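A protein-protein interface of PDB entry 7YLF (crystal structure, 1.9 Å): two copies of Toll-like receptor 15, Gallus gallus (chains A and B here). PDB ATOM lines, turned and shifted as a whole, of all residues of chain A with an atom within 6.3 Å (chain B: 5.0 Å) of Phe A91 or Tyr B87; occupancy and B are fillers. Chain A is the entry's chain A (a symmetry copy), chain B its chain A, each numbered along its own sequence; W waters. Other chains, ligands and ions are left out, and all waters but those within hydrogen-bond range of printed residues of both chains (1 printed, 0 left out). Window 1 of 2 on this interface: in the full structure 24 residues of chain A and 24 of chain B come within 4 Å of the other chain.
The side-chain amide oxygen (OE1) of Gln B86 is in hydrogen-bond range of the backbone NH (N) of Ile A61, at 3.0 Å. OH of Tyr B87 is in hydrogen-bond range of NE2 of His A47 (3.1 Å). OE2 of Glu B88 sits close to OH of Tyr A87, at 2.4 Å. The side-chain hydroxyl (OH) of Tyr B87 lies close to the side-chain carboxylate (OE2) of Glu A88 (2.4 Å).
OG of Ser A20 lies within hydrogen-bond range of OE1 of Glu A88 (2.6 Å). The backbone carbonyl oxygen (O) of Tyr A90 lies within hydrogen-bond range of a ring nitrogen (ND1) of His A94 (3.0 Å).
Among the printed residues, pairs that only touch across the chains: Trp A84 with CME B85 (3.3 Å), Arg A95 with Tyr B90 (3.4 Å), Tyr A87 with Phe B91 (3.4 Å), Phe A91 with Tyr B87 (3.4 Å), His A94 with Tyr B90 (3.5 Å), His A47 with Cys B83 (3.6 Å), Ile A61 with Cys B83 (3.6 Å), Phe A91 with Tyr B90 (3.7 Å), Tyr A90 with Phe B91 (3.7 Å), Phe A18 with Tyr B87 (3.7 Å), Ile A61 with Tyr B87 (3.7 Å), Tyr A87 with Tyr B87 (3.8 Å), Trp A84 with Trp B84 (3.9 Å), Phe A62 with Tyr B90 (3.95 Å) and Tyr A90 with Tyr B90 (3.98 Å).
Of the printed residues of chain B, His A47 touches Cys B83 and Tyr B87. Gln A86 touches none of the printed residues of chain B. Leu A89 touches none of the printed residues of chain B. Of chain B, only Tyr B87 (3.4 Å) and Tyr B90 (3.7 Å) come within 4 Å of Phe A91. Of the printed residues of chain A, CME B85 touches Trp A84 (3.3 Å). Of chain A, only Phe A18 (3.7 Å), His A47 (3.1 Å), Ile A61 (3.7 Å), Tyr A87 (3.8 Å), Glu A88 (2.4 Å) and Phe A91 (3.4 Å) come within 4 Å of Tyr B87. Of the printed residues of chain A, Glu B88 touches Tyr A87. The nearest printed residue of chain A that does not touch Tyr B87 is Trp A84 (5.6 Å).
Hydrophobic or aromatic side chains of chain A that line the printed part of chain B: Phe A18, His A47, Ile A61, Phe A62, Trp A84, Tyr A87, Tyr A90, Phe A91 and His A94. Hydrophobic or aromatic side chains of chain B that line the printed part of chain A: Trp B84, Tyr B87, Tyr B90 and Phe B91. Among the printed residues, no Asp or Glu carboxylate lies within 4 Å of a Lys or Arg side-chain nitrogen of the other chain.
Trp B84 touches its own counterpart, Trp A84. Tyr A87 touches its own counterpart, Tyr B87. Tyr A87 touches Glu B88, and with the chains exchanged Glu A88 touches Tyr B87. Tyr A90 touches Phe B91, and with the chains exchanged Phe A91 touches Tyr B90. Positions printed for both chains: 84, 86, 87, 88, 89, 90 and 91. Of the 19 pairs that touch across the chains among the printed residues, 9 have their exchanged pair printed and touching as well.
Water W1 lies within hydrogen-bond range of the backbone carbonyl oxygen (O) of Tyr B87 (3.1 Å) and the backbone carbonyl oxygen (O) of Tyr A87 (3.1 Å).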
ATOM      1  N   PHE A  18     -10.939 -12.436  22.342  1.00  0.00           N
ATOM      2  CA  PHE A  18     -10.731 -11.006  22.518  1.00  0.00           C
ATOM      3  C   PHE A  18     -10.384 -10.774  23.984  1.00  0.00           C
ATOM      4  O   PHE A  18     -11.142 -11.179  24.874  1.00  0.00           O
ATOM      5  CB  PHE A  18     -12.004 -10.247  22.120  1.00  0.00           C
ATOM      6  CG  PHE A  18     -12.071  -8.828  22.632  1.00  0.00           C
ATOM      7  CD1 PHE A  18     -11.064  -7.918  22.334  1.00  0.00           C
ATOM      8  CD2 PHE A  18     -13.158  -8.403  23.395  1.00  0.00           C
ATOM      9  CE1 PHE A  18     -11.128  -6.597  22.801  1.00  0.00           C
ATOM     10  CE2 PHE A  18     -13.231  -7.082  23.860  1.00  0.00           C
ATOM     11  CZ  PHE A  18     -12.211  -6.187  23.559  1.00  0.00           C
ATOM     12  N   SER A  20      -9.335  -8.220  27.193  1.00  0.00           N
ATOM     13  CA  SER A  20      -9.385  -6.852  27.696  1.00  0.00           C
ATOM     14  C   SER A  20      -8.769  -6.797  29.089  1.00  0.00           C
ATOM     15  O   SER A  20      -8.973  -7.704  29.907  1.00  0.00           O
ATOM     16  CB  SER A  20     -10.823  -6.349  27.724  1.00  0.00           C
ATOM     17  OG  SER A  20     -11.031  -5.486  28.822  1.00  0.00           O
ATOM     18  N   HIS A  47      -7.075  -4.716  21.555  1.00  0.00           N
ATOM     19  CA  HIS A  47      -7.141  -3.414  20.892  1.00  0.00           C
ATOM     20  C   HIS A  47      -5.789  -2.722  20.859  1.00  0.00           C
ATOM     21  O   HIS A  47      -5.474  -2.015  19.893  1.00  0.00           O
ATOM     22  CB  HIS A  47      -8.170  -2.510  21.586  1.00  0.00           C
ATOM     23  CG  HIS A  47      -9.593  -2.903  21.332  1.00  0.00           C
ATOM     24  ND1 HIS A  47      -9.996  -3.571  20.193  1.00  0.00           N
ATOM     25  CD2 HIS A  47     -10.708  -2.729  22.077  1.00  0.00           C
ATOM     26  CE1 HIS A  47     -11.301  -3.779  20.246  1.00  0.00           C
ATOM     27  NE2 HIS A  47     -11.751  -3.296  21.390  1.00  0.00           N
ATOM     28  N   ILE A  61     -14.776  -1.039  17.440  1.00  0.00           N
ATOM     29  CA  ILE A  61     -14.743  -1.911  18.607  1.00  0.00           C
ATOM     30  C   ILE A  61     -15.485  -3.218  18.397  1.00  0.00           C
ATOM     31  O   ILE A  61     -15.373  -4.116  19.239  1.00  0.00           O
ATOM     32  CB  ILE A  61     -15.341  -1.193  19.835  1.00  0.00           C
ATOM     33  CG1 ILE A  61     -16.740  -0.661  19.522  1.00  0.00           C
ATOM     34  CG2 ILE A  61     -14.456  -0.008  20.259  1.00  0.00           C
ATOM     35  CD1 ILE A  61     -17.497  -0.269  20.787  1.00  0.00           C
ATOM     36  N   PHE A  62     -16.269  -3.339  17.327  1.00  0.00           N
ATOM     37  CA  PHE A  62     -16.989  -4.585  17.097  1.00  0.00           C
ATOM     38  C   PHE A  62     -16.113  -5.655  16.466  1.00  0.00           C
ATOM     39  O   PHE A  62     -16.469  -6.842  16.518  1.00  0.00           O
ATOM     40  CB  PHE A  62     -18.202  -4.332  16.204  1.00  0.00           C
ATOM     41  CG  PHE A  62     -19.219  -3.408  16.830  1.00  0.00           C
ATOM     42  CD1 PHE A  62     -20.160  -3.900  17.713  1.00  0.00           C
ATOM     43  CD2 PHE A  62     -19.209  -2.059  16.546  1.00  0.00           C
ATOM     44  CE1 PHE A  62     -21.095  -3.049  18.295  1.00  0.00           C
ATOM     45  CE2 PHE A  62     -20.131  -1.216  17.120  1.00  0.00           C
ATOM     46  CZ  PHE A  62     -21.073  -1.725  18.003  1.00  0.00           C
ATOM     47  N   ILE A  65     -14.503  -8.564  19.025  1.00  0.00           N
ATOM     48  CA  ILE A  65     -15.496  -9.385  19.712  1.00  0.00           C
ATOM     49  C   ILE A  65     -16.301 -10.202  18.712  1.00  0.00           C
ATOM     50  O   ILE A  65     -16.628 -11.371  18.964  1.00  0.00           O
ATOM     51  CB  ILE A  65     -16.391  -8.506  20.611  1.00  0.00           C
ATOM     52  CG1 ILE A  65     -17.235  -9.366  21.556  1.00  0.00           C
ATOM     53  CG2 ILE A  65     -17.270  -7.574  19.780  1.00  0.00           C
ATOM     54  CD1 ILE A  65     -17.832  -8.579  22.707  1.00  0.00           C
ATOM     55  N   TRP A  84     -12.635   3.418  31.864  1.00  0.00           N
ATOM     56  CA  TRP A  84     -12.571   2.772  30.553  1.00  0.00           C
ATOM     57  C   TRP A  84     -12.931   1.301  30.612  1.00  0.00           C
ATOM     58  O   TRP A  84     -13.632   0.790  29.737  1.00  0.00           O
ATOM     59  CB  TRP A  84     -11.184   2.959  29.940  1.00  0.00           C
ATOM     60  CG  TRP A  84     -10.872   4.403  29.763  1.00  0.00           C
ATOM     61  CD1 TRP A  84      -9.756   5.061  30.188  1.00  0.00           C
ATOM     62  CD2 TRP A  84     -11.719   5.392  29.159  1.00  0.00           C
ATOM     63  NE1 TRP A  84      -9.840   6.392  29.859  1.00  0.00           N
ATOM     64  CE2 TRP A  84     -11.037   6.621  29.231  1.00  0.00           C
ATOM     65  CE3 TRP A  84     -12.976   5.353  28.545  1.00  0.00           C
ATOM     66  CZ2 TRP A  84     -11.574   7.802  28.721  1.00  0.00           C
ATOM     67  CZ3 TRP A  84     -13.509   6.527  28.044  1.00  0.00           C
ATOM     68  CH2 TRP A  84     -12.810   7.732  28.134  1.00  0.00           C
ATOM     69  N   GLN A  86     -14.925  -0.066  32.764  1.00  0.00           N
ATOM     70  CA  GLN A  86     -16.346  -0.203  32.998  1.00  0.00           C
ATOM     71  C   GLN A  86     -17.102  -0.076  31.660  1.00  0.00           C
ATOM     72  O   GLN A  86     -18.089  -0.760  31.440  1.00  0.00           O
ATOM     73  CB  GLN A  86     -16.836   0.852  34.019  1.00  0.00           C
ATOM     74  CG  GLN A  86     -16.362   0.505  35.447  1.00  0.00           C
ATOM     75  CD  GLN A  86     -16.900   1.498  36.472  1.00  0.00           C
ATOM     76  OE1 GLN A  86     -17.875   2.185  36.207  1.00  0.00           O
ATOM     77  NE2 GLN A  86     -16.270   1.562  37.643  1.00  0.00           N
ATOM     78  N   TYR A  87     -16.635   0.805  30.775  1.00  0.00           N
ATOM     79  CA  TYR A  87     -17.230   0.882  29.440  1.00  0.00           C
ATOM     80  C   TYR A  87     -17.022  -0.419  28.679  1.00  0.00           C
ATOM     81  O   TYR A  87     -17.920  -0.886  27.969  1.00  0.00           O
ATOM     82  CB  TYR A  87     -16.618   2.032  28.648  1.00  0.00           C
ATOM     83  CG  TYR A  87     -17.224   3.377  28.950  1.00  0.00           C
ATOM     84  CD1 TYR A  87     -18.537   3.645  28.621  1.00  0.00           C
ATOM     85  CD2 TYR A  87     -16.479   4.382  29.548  1.00  0.00           C
ATOM     86  CE1 TYR A  87     -19.106   4.890  28.889  1.00  0.00           C
ATOM     87  CE2 TYR A  87     -17.039   5.626  29.824  1.00  0.00           C
ATOM     88  CZ  TYR A  87     -18.351   5.867  29.499  1.00  0.00           C
ATOM     89  OH  TYR A  87     -18.928   7.098  29.745  1.00  0.00           O
ATOM     90  N   GLU A  88     -15.831  -1.000  28.792  1.00  0.00           N
ATOM     91  CA  GLU A  88     -15.582  -2.274  28.112  1.00  0.00           C
ATOM     92  C   GLU A  88     -16.484  -3.366  28.679  1.00  0.00           C
ATOM     93  O   GLU A  88     -17.081  -4.138  27.920  1.00  0.00           O
ATOM     94  CB  GLU A  88     -14.099  -2.650  28.212  1.00  0.00           C
ATOM     95  CG  GLU A  88     -13.618  -3.734  27.175  1.00  0.00           C
ATOM     96  CD  GLU A  88     -12.259  -3.389  26.577  1.00  0.00           C
ATOM     97  OE1 GLU A  88     -11.261  -3.371  27.324  1.00  0.00           O
ATOM     98  OE2 GLU A  88     -12.182  -3.098  25.367  1.00  0.00           O
ATOM     99  N   LEU A  89     -16.646  -3.404  30.006  1.00  0.00           N
ATOM    100  CA  LEU A  89     -17.552  -4.372  30.622  1.00  0.00           C
ATOM    101  C   LEU A  89     -18.978  -4.192  30.125  1.00  0.00           C
ATOM    102  O   LEU A  89     -19.662  -5.172  29.813  1.00  0.00           O
ATOM    103  CB  LEU A  89     -17.536  -4.236  32.141  1.00  0.00           C
ATOM    104  CG  LEU A  89     -16.783  -5.201  33.043  1.00  0.00           C
ATOM    105  CD1 LEU A  89     -17.093  -4.793  34.478  1.00  0.00           C
ATOM    106  CD2 LEU A  89     -17.134  -6.684  32.775  1.00  0.00           C
ATOM    107  N   TYR A  90     -19.456  -2.940  30.087  1.00  0.00           N
ATOM    108  CA  TYR A  90     -20.808  -2.668  29.598  1.00  0.00           C
ATOM    109  C   TYR A  90     -21.001  -3.240  28.196  1.00  0.00           C
ATOM    110  O   TYR A  90     -22.008  -3.899  27.904  1.00  0.00           O
ATOM    111  CB  TYR A  90     -21.067  -1.159  29.594  1.00  0.00           C
ATOM    112  CG  TYR A  90     -22.489  -0.815  29.234  1.00  0.00           C
ATOM    113  CD1 TYR A  90     -23.480  -0.765  30.208  1.00  0.00           C
ATOM    114  CD2 TYR A  90     -22.847  -0.560  27.916  1.00  0.00           C
ATOM    115  CE1 TYR A  90     -24.788  -0.465  29.875  1.00  0.00           C
ATOM    116  CE2 TYR A  90     -24.151  -0.275  27.574  1.00  0.00           C
ATOM    117  CZ  TYR A  90     -25.115  -0.224  28.556  1.00  0.00           C
ATOM    118  OH  TYR A  90     -26.417   0.078  28.220  1.00  0.00           O
ATOM    119  N   PHE A  91     -20.029  -2.992  27.320  1.00  0.00           N
ATOM    120  CA  PHE A  91     -20.112  -3.437  25.930  1.00  0.00           C
ATOM    121  C   PHE A  91     -20.196  -4.956  25.843  1.00  0.00           C
ATOM    122  O   PHE A  91     -21.089  -5.521  25.189  1.00  0.00           O
ATOM    123  CB  PHE A  91     -18.882  -2.903  25.190  1.00  0.00           C
ATOM    124  CG  PHE A  91     -18.771  -3.339  23.758  1.00  0.00           C
ATOM    125  CD1 PHE A  91     -19.637  -2.841  22.806  1.00  0.00           C
ATOM    126  CD2 PHE A  91     -17.756  -4.191  23.356  1.00  0.00           C
ATOM    127  CE1 PHE A  91     -19.527  -3.209  21.488  1.00  0.00           C
ATOM    128  CE2 PHE A  91     -17.636  -4.556  22.032  1.00  0.00           C
ATOM    129  CZ  PHE A  91     -18.527  -4.067  21.100  1.00  0.00           C
ATOM    130  N   ALA A  92     -19.286  -5.644  26.519  1.00  0.00           N
ATOM    131  CA  ALA A  92     -19.286  -7.096  26.425  1.00  0.00           C
ATOM    132  C   ALA A  92     -20.540  -7.674  27.061  1.00  0.00           C
ATOM    133  O   ALA A  92     -21.169  -8.575  26.492  1.00  0.00           O
ATOM    134  CB  ALA A  92     -18.034  -7.663  27.079  1.00  0.00           C
ATOM    135  N   GLU A  93     -20.935  -7.146  28.225  1.00  0.00           N
ATOM    136  CA  GLU A  93     -22.162  -7.601  28.871  1.00  0.00           C
ATOM    137  C   GLU A  93     -23.365  -7.479  27.943  1.00  0.00           C
ATOM    138  O   GLU A  93     -24.225  -8.365  27.916  1.00  0.00           O
ATOM    139  CB  GLU A  93     -22.409  -6.816  30.160  1.00  0.00           C
ATOM    140  CG  GLU A  93     -21.461  -7.197  31.298  1.00  0.00           C
ATOM    141  CD  GLU A  93     -22.108  -7.126  32.675  1.00  0.00           C
ATOM    142  OE1 GLU A  93     -23.311  -6.789  32.768  1.00  0.00           O
ATOM    143  OE2 GLU A  93     -21.408  -7.427  33.667  1.00  0.00           O
ATOM    144  N   HIS A  94     -23.450  -6.393  27.177  1.00  0.00           N
ATOM    145  CA  HIS A  94     -24.604  -6.200  26.307  1.00  0.00           C
ATOM    146  C   HIS A  94     -24.430  -6.839  24.940  1.00  0.00           C
ATOM    147  O   HIS A  94     -25.426  -7.205  24.308  1.00  0.00           O
ATOM    148  CB  HIS A  94     -24.906  -4.705  26.162  1.00  0.00           C
ATOM    149  CG  HIS A  94     -25.576  -4.127  27.363  1.00  0.00           C
ATOM    150  ND1 HIS A  94     -24.958  -4.056  28.594  1.00  0.00           N
ATOM    151  CD2 HIS A  94     -26.824  -3.633  27.540  1.00  0.00           C
ATOM    152  CE1 HIS A  94     -25.791  -3.531  29.472  1.00  0.00           C
ATOM    153  NE2 HIS A  94     -26.930  -3.263  28.859  1.00  0.00           N
ATOM    154  N   ARG A  95     -23.195  -6.989  24.466  1.00  0.00           N
ATOM    155  CA  ARG A  95     -22.970  -7.766  23.254  1.00  0.00           C
ATOM    156  C   ARG A  95     -22.997  -9.266  23.533  1.00  0.00           C
ATOM    157  O   ARG A  95     -23.632 -10.020  22.791  1.00  0.00           O
ATOM    158  CB  ARG A  95     -21.642  -7.370  22.608  1.00  0.00           C
ATOM    159  CG  ARG A  95     -21.607  -5.951  22.075  1.00  0.00           C
ATOM    160  CD  ARG A  95     -22.564  -5.768  20.911  1.00  0.00           C
ATOM    161  NE  ARG A  95     -22.267  -6.672  19.804  1.00  0.00           N
ATOM    162  CZ  ARG A  95     -22.883  -6.638  18.625  1.00  0.00           C
ATOM    163  NH1 ARG A  95     -23.831  -5.742  18.395  1.00  0.00           N
ATOM    164  NH2 ARG A  95     -22.549  -7.498  17.674  1.00  0.00           N
ATOM    165  N   VAL A  96     -22.321  -9.717  24.591  1.00  0.00           N
ATOM    166  CA  VAL A  96     -22.251 -11.145  24.920  1.00  0.00           C
ATOM    167  C   VAL A  96     -23.035 -11.452  26.191  1.00  0.00           C
ATOM    168  O   VAL A  96     -24.267 -11.418  26.199  1.00  0.00           O
ATOM    169  CB  VAL A  96     -20.792 -11.611  25.073  1.00  0.00           C
ATOM    170  N   CYS B  83     -11.053   4.353  19.900  1.00  0.00           N
ATOM    171  CA  CYS B  83     -11.590   3.159  20.538  1.00  0.00           C
ATOM    172  C   CYS B  83     -12.418   3.519  21.770  1.00  0.00           C
ATOM    173  O   CYS B  83     -13.557   3.062  21.939  1.00  0.00           O
ATOM    174  CB  CYS B  83     -10.420   2.245  20.909  1.00  0.00           C
ATOM    175  SG  CYS B  83     -10.843   0.838  21.872  1.00  0.00           S
ATOM    176  N   TRP B  84     -11.876   4.371  22.622  1.00  0.00           N
ATOM    177  CA  TRP B  84     -12.574   4.742  23.852  1.00  0.00           C
ATOM    178  C   TRP B  84     -13.858   5.504  23.585  1.00  0.00           C
ATOM    179  O   TRP B  84     -14.874   5.272  24.243  1.00  0.00           O
ATOM    180  CB  TRP B  84     -11.650   5.555  24.758  1.00  0.00           C
ATOM    181  CG  TRP B  84     -10.442   4.767  25.128  1.00  0.00           C
ATOM    182  CD1 TRP B  84      -9.140   5.154  25.008  1.00  0.00           C
ATOM    183  CD2 TRP B  84     -10.420   3.422  25.627  1.00  0.00           C
ATOM    184  NE1 TRP B  84      -8.309   4.147  25.432  1.00  0.00           N
ATOM    185  CE2 TRP B  84      -9.070   3.071  25.812  1.00  0.00           C
ATOM    186  CE3 TRP B  84     -11.411   2.489  25.956  1.00  0.00           C
ATOM    187  CZ2 TRP B  84      -8.685   1.825  26.303  1.00  0.00           C
ATOM    188  CZ3 TRP B  84     -11.025   1.251  26.438  1.00  0.00           C
ATOM    189  CH2 TRP B  84      -9.677   0.932  26.608  1.00  0.00           C
ATOM    190  N   CME B  85     -13.829   6.394  22.606  1.00  0.00           N
ATOM    191  CA  CME B  85     -15.046   7.178  22.271  1.00  0.00           C
ATOM    192  CB  CME B  85     -14.715   8.341  21.373  1.00  0.00           C
ATOM    193  SG  CME B  85     -13.661   9.604  22.132  1.00  0.00           S
ATOM    194  SD  CME B  85     -14.637  10.151  23.829  1.00  0.00           S
ATOM    195  CE  CME B  85     -13.931   9.051  25.092  1.00  0.00           C
ATOM    196  CZ  CME B  85     -12.458   9.317  25.213  1.00  0.00           C
ATOM    197  OH  CME B  85     -12.168  10.643  25.627  1.00  0.00           O
ATOM    198  C   CME B  85     -16.104   6.254  21.662  1.00  0.00           C
ATOM    199  O   CME B  85     -17.301   6.535  21.856  1.00  0.00           O
ATOM    200  N   GLN B  86     -15.709   5.210  20.947  1.00  0.00           N
ATOM    201  CA  GLN B  86     -16.700   4.303  20.407  1.00  0.00           C
ATOM    202  C   GLN B  86     -17.391   3.550  21.562  1.00  0.00           C
ATOM    203  O   GLN B  86     -18.584   3.293  21.506  1.00  0.00           O
ATOM    204  CB  GLN B  86     -16.051   3.317  19.407  1.00  0.00           C
ATOM    205  CG  GLN B  86     -15.686   4.026  18.085  1.00  0.00           C
ATOM    206  CD  GLN B  86     -15.113   3.048  17.064  1.00  0.00           C
ATOM    207  OE1 GLN B  86     -15.322   1.851  17.179  1.00  0.00           O
ATOM    208  NE2 GLN B  86     -14.403   3.564  16.063  1.00  0.00           N
ATOM    209  N   TYR B  87     -16.634   3.198  22.602  1.00  0.00           N
ATOM    210  CA  TYR B  87     -17.255   2.597  23.783  1.00  0.00           C
ATOM    211  C   TYR B  87     -18.212   3.573  24.449  1.00  0.00           C
ATOM    212  O   TYR B  87     -19.292   3.185  24.909  1.00  0.00           O
ATOM    213  CB  TYR B  87     -16.189   2.172  24.788  1.00  0.00           C
ATOM    214  CG  TYR B  87     -15.561   0.837  24.488  1.00  0.00           C
ATOM    215  CD1 TYR B  87     -16.307  -0.323  24.557  1.00  0.00           C
ATOM    216  CD2 TYR B  87     -14.219   0.733  24.154  1.00  0.00           C
ATOM    217  CE1 TYR B  87     -15.734  -1.564  24.289  1.00  0.00           C
ATOM    218  CE2 TYR B  87     -13.638  -0.503  23.881  1.00  0.00           C
ATOM    219  CZ  TYR B  87     -14.403  -1.641  23.943  1.00  0.00           C
ATOM    220  OH  TYR B  87     -13.849  -2.882  23.694  1.00  0.00           O
ATOM    221  N   GLU B  88     -17.817   4.841  24.538  1.00  0.00           N
ATOM    222  CA  GLU B  88     -18.710   5.835  25.135  1.00  0.00           C
ATOM    223  C   GLU B  88     -19.973   5.991  24.294  1.00  0.00           C
ATOM    224  O   GLU B  88     -21.083   6.026  24.837  1.00  0.00           O
ATOM    225  CB  GLU B  88     -17.976   7.169  25.316  1.00  0.00           C
ATOM    226  CG  GLU B  88     -18.655   8.169  26.329  1.00  0.00           C
ATOM    227  CD  GLU B  88     -17.632   8.853  27.228  1.00  0.00           C
ATOM    228  OE1 GLU B  88     -16.801   9.626  26.712  1.00  0.00           O
ATOM    229  OE2 GLU B  88     -17.627   8.597  28.448  1.00  0.00           O
ATOM    230  N   LEU B  89     -19.828   6.023  22.965  1.00  0.00           N
ATOM    231  CA  LEU B  89     -20.995   6.094  22.086  1.00  0.00           C
ATOM    232  C   LEU B  89     -21.915   4.900  22.287  1.00  0.00           C
ATOM    233  O   LEU B  89     -23.138   5.056  22.357  1.00  0.00           O
ATOM    234  CB  LEU B  89     -20.567   6.151  20.623  1.00  0.00           C
ATOM    235  CG  LEU B  89     -20.571   7.439  19.817  1.00  0.00           C
ATOM    236  CD1 LEU B  89     -20.182   7.066  18.392  1.00  0.00           C
ATOM    237  CD2 LEU B  89     -21.926   8.184  19.869  1.00  0.00           C
ATOM    238  N   TYR B  90     -21.340   3.690  22.337  1.00  0.00           N
ATOM    239  CA  TYR B  90     -22.144   2.488  22.553  1.00  0.00           C
ATOM    240  C   TYR B  90     -22.979   2.615  23.825  1.00  0.00           C
ATOM    241  O   TYR B  90     -24.181   2.320  23.837  1.00  0.00           O
ATOM    242  CB  TYR B  90     -21.232   1.260  22.640  1.00  0.00           C
ATOM    243  CG  TYR B  90     -22.003  -0.032  22.721  1.00  0.00           C
ATOM    244  CD1 TYR B  90     -22.419  -0.689  21.570  1.00  0.00           C
ATOM    245  CD2 TYR B  90     -22.334  -0.586  23.952  1.00  0.00           C
ATOM    246  CE1 TYR B  90     -23.141  -1.866  21.646  1.00  0.00           C
ATOM    247  CE2 TYR B  90     -23.066  -1.749  24.037  1.00  0.00           C
ATOM    248  CZ  TYR B  90     -23.462  -2.389  22.883  1.00  0.00           C
ATOM    249  OH  TYR B  90     -24.177  -3.563  22.963  1.00  0.00           O
ATOM    250  N   PHE B  91     -22.340   3.063  24.904  1.00  0.00           N
ATOM    251  CA  PHE B  91     -23.007   3.184  26.200  1.00  0.00           C
ATOM    252  C   PHE B  91     -24.174   4.162  26.129  1.00  0.00           C
ATOM    253  O   PHE B  91     -25.309   3.851  26.526  1.00  0.00           O
ATOM    254  CB  PHE B  91     -21.965   3.633  27.228  1.00  0.00           C
ATOM    255  CG  PHE B  91     -22.506   3.881  28.605  1.00  0.00           C
ATOM    256  CD1 PHE B  91     -22.922   2.830  29.394  1.00  0.00           C
ATOM    257  CD2 PHE B  91     -22.529   5.162  29.133  1.00  0.00           C
ATOM    258  CE1 PHE B  91     -23.391   3.043  30.668  1.00  0.00           C
ATOM    259  CE2 PHE B  91     -22.991   5.379  30.413  1.00  0.00           C
ATOM    260  CZ  PHE B  91     -23.426   4.317  31.177  1.00  0.00           C
HETATM  261  O   HOH W   1     -20.029   0.535  26.259  1.00  0.00           O
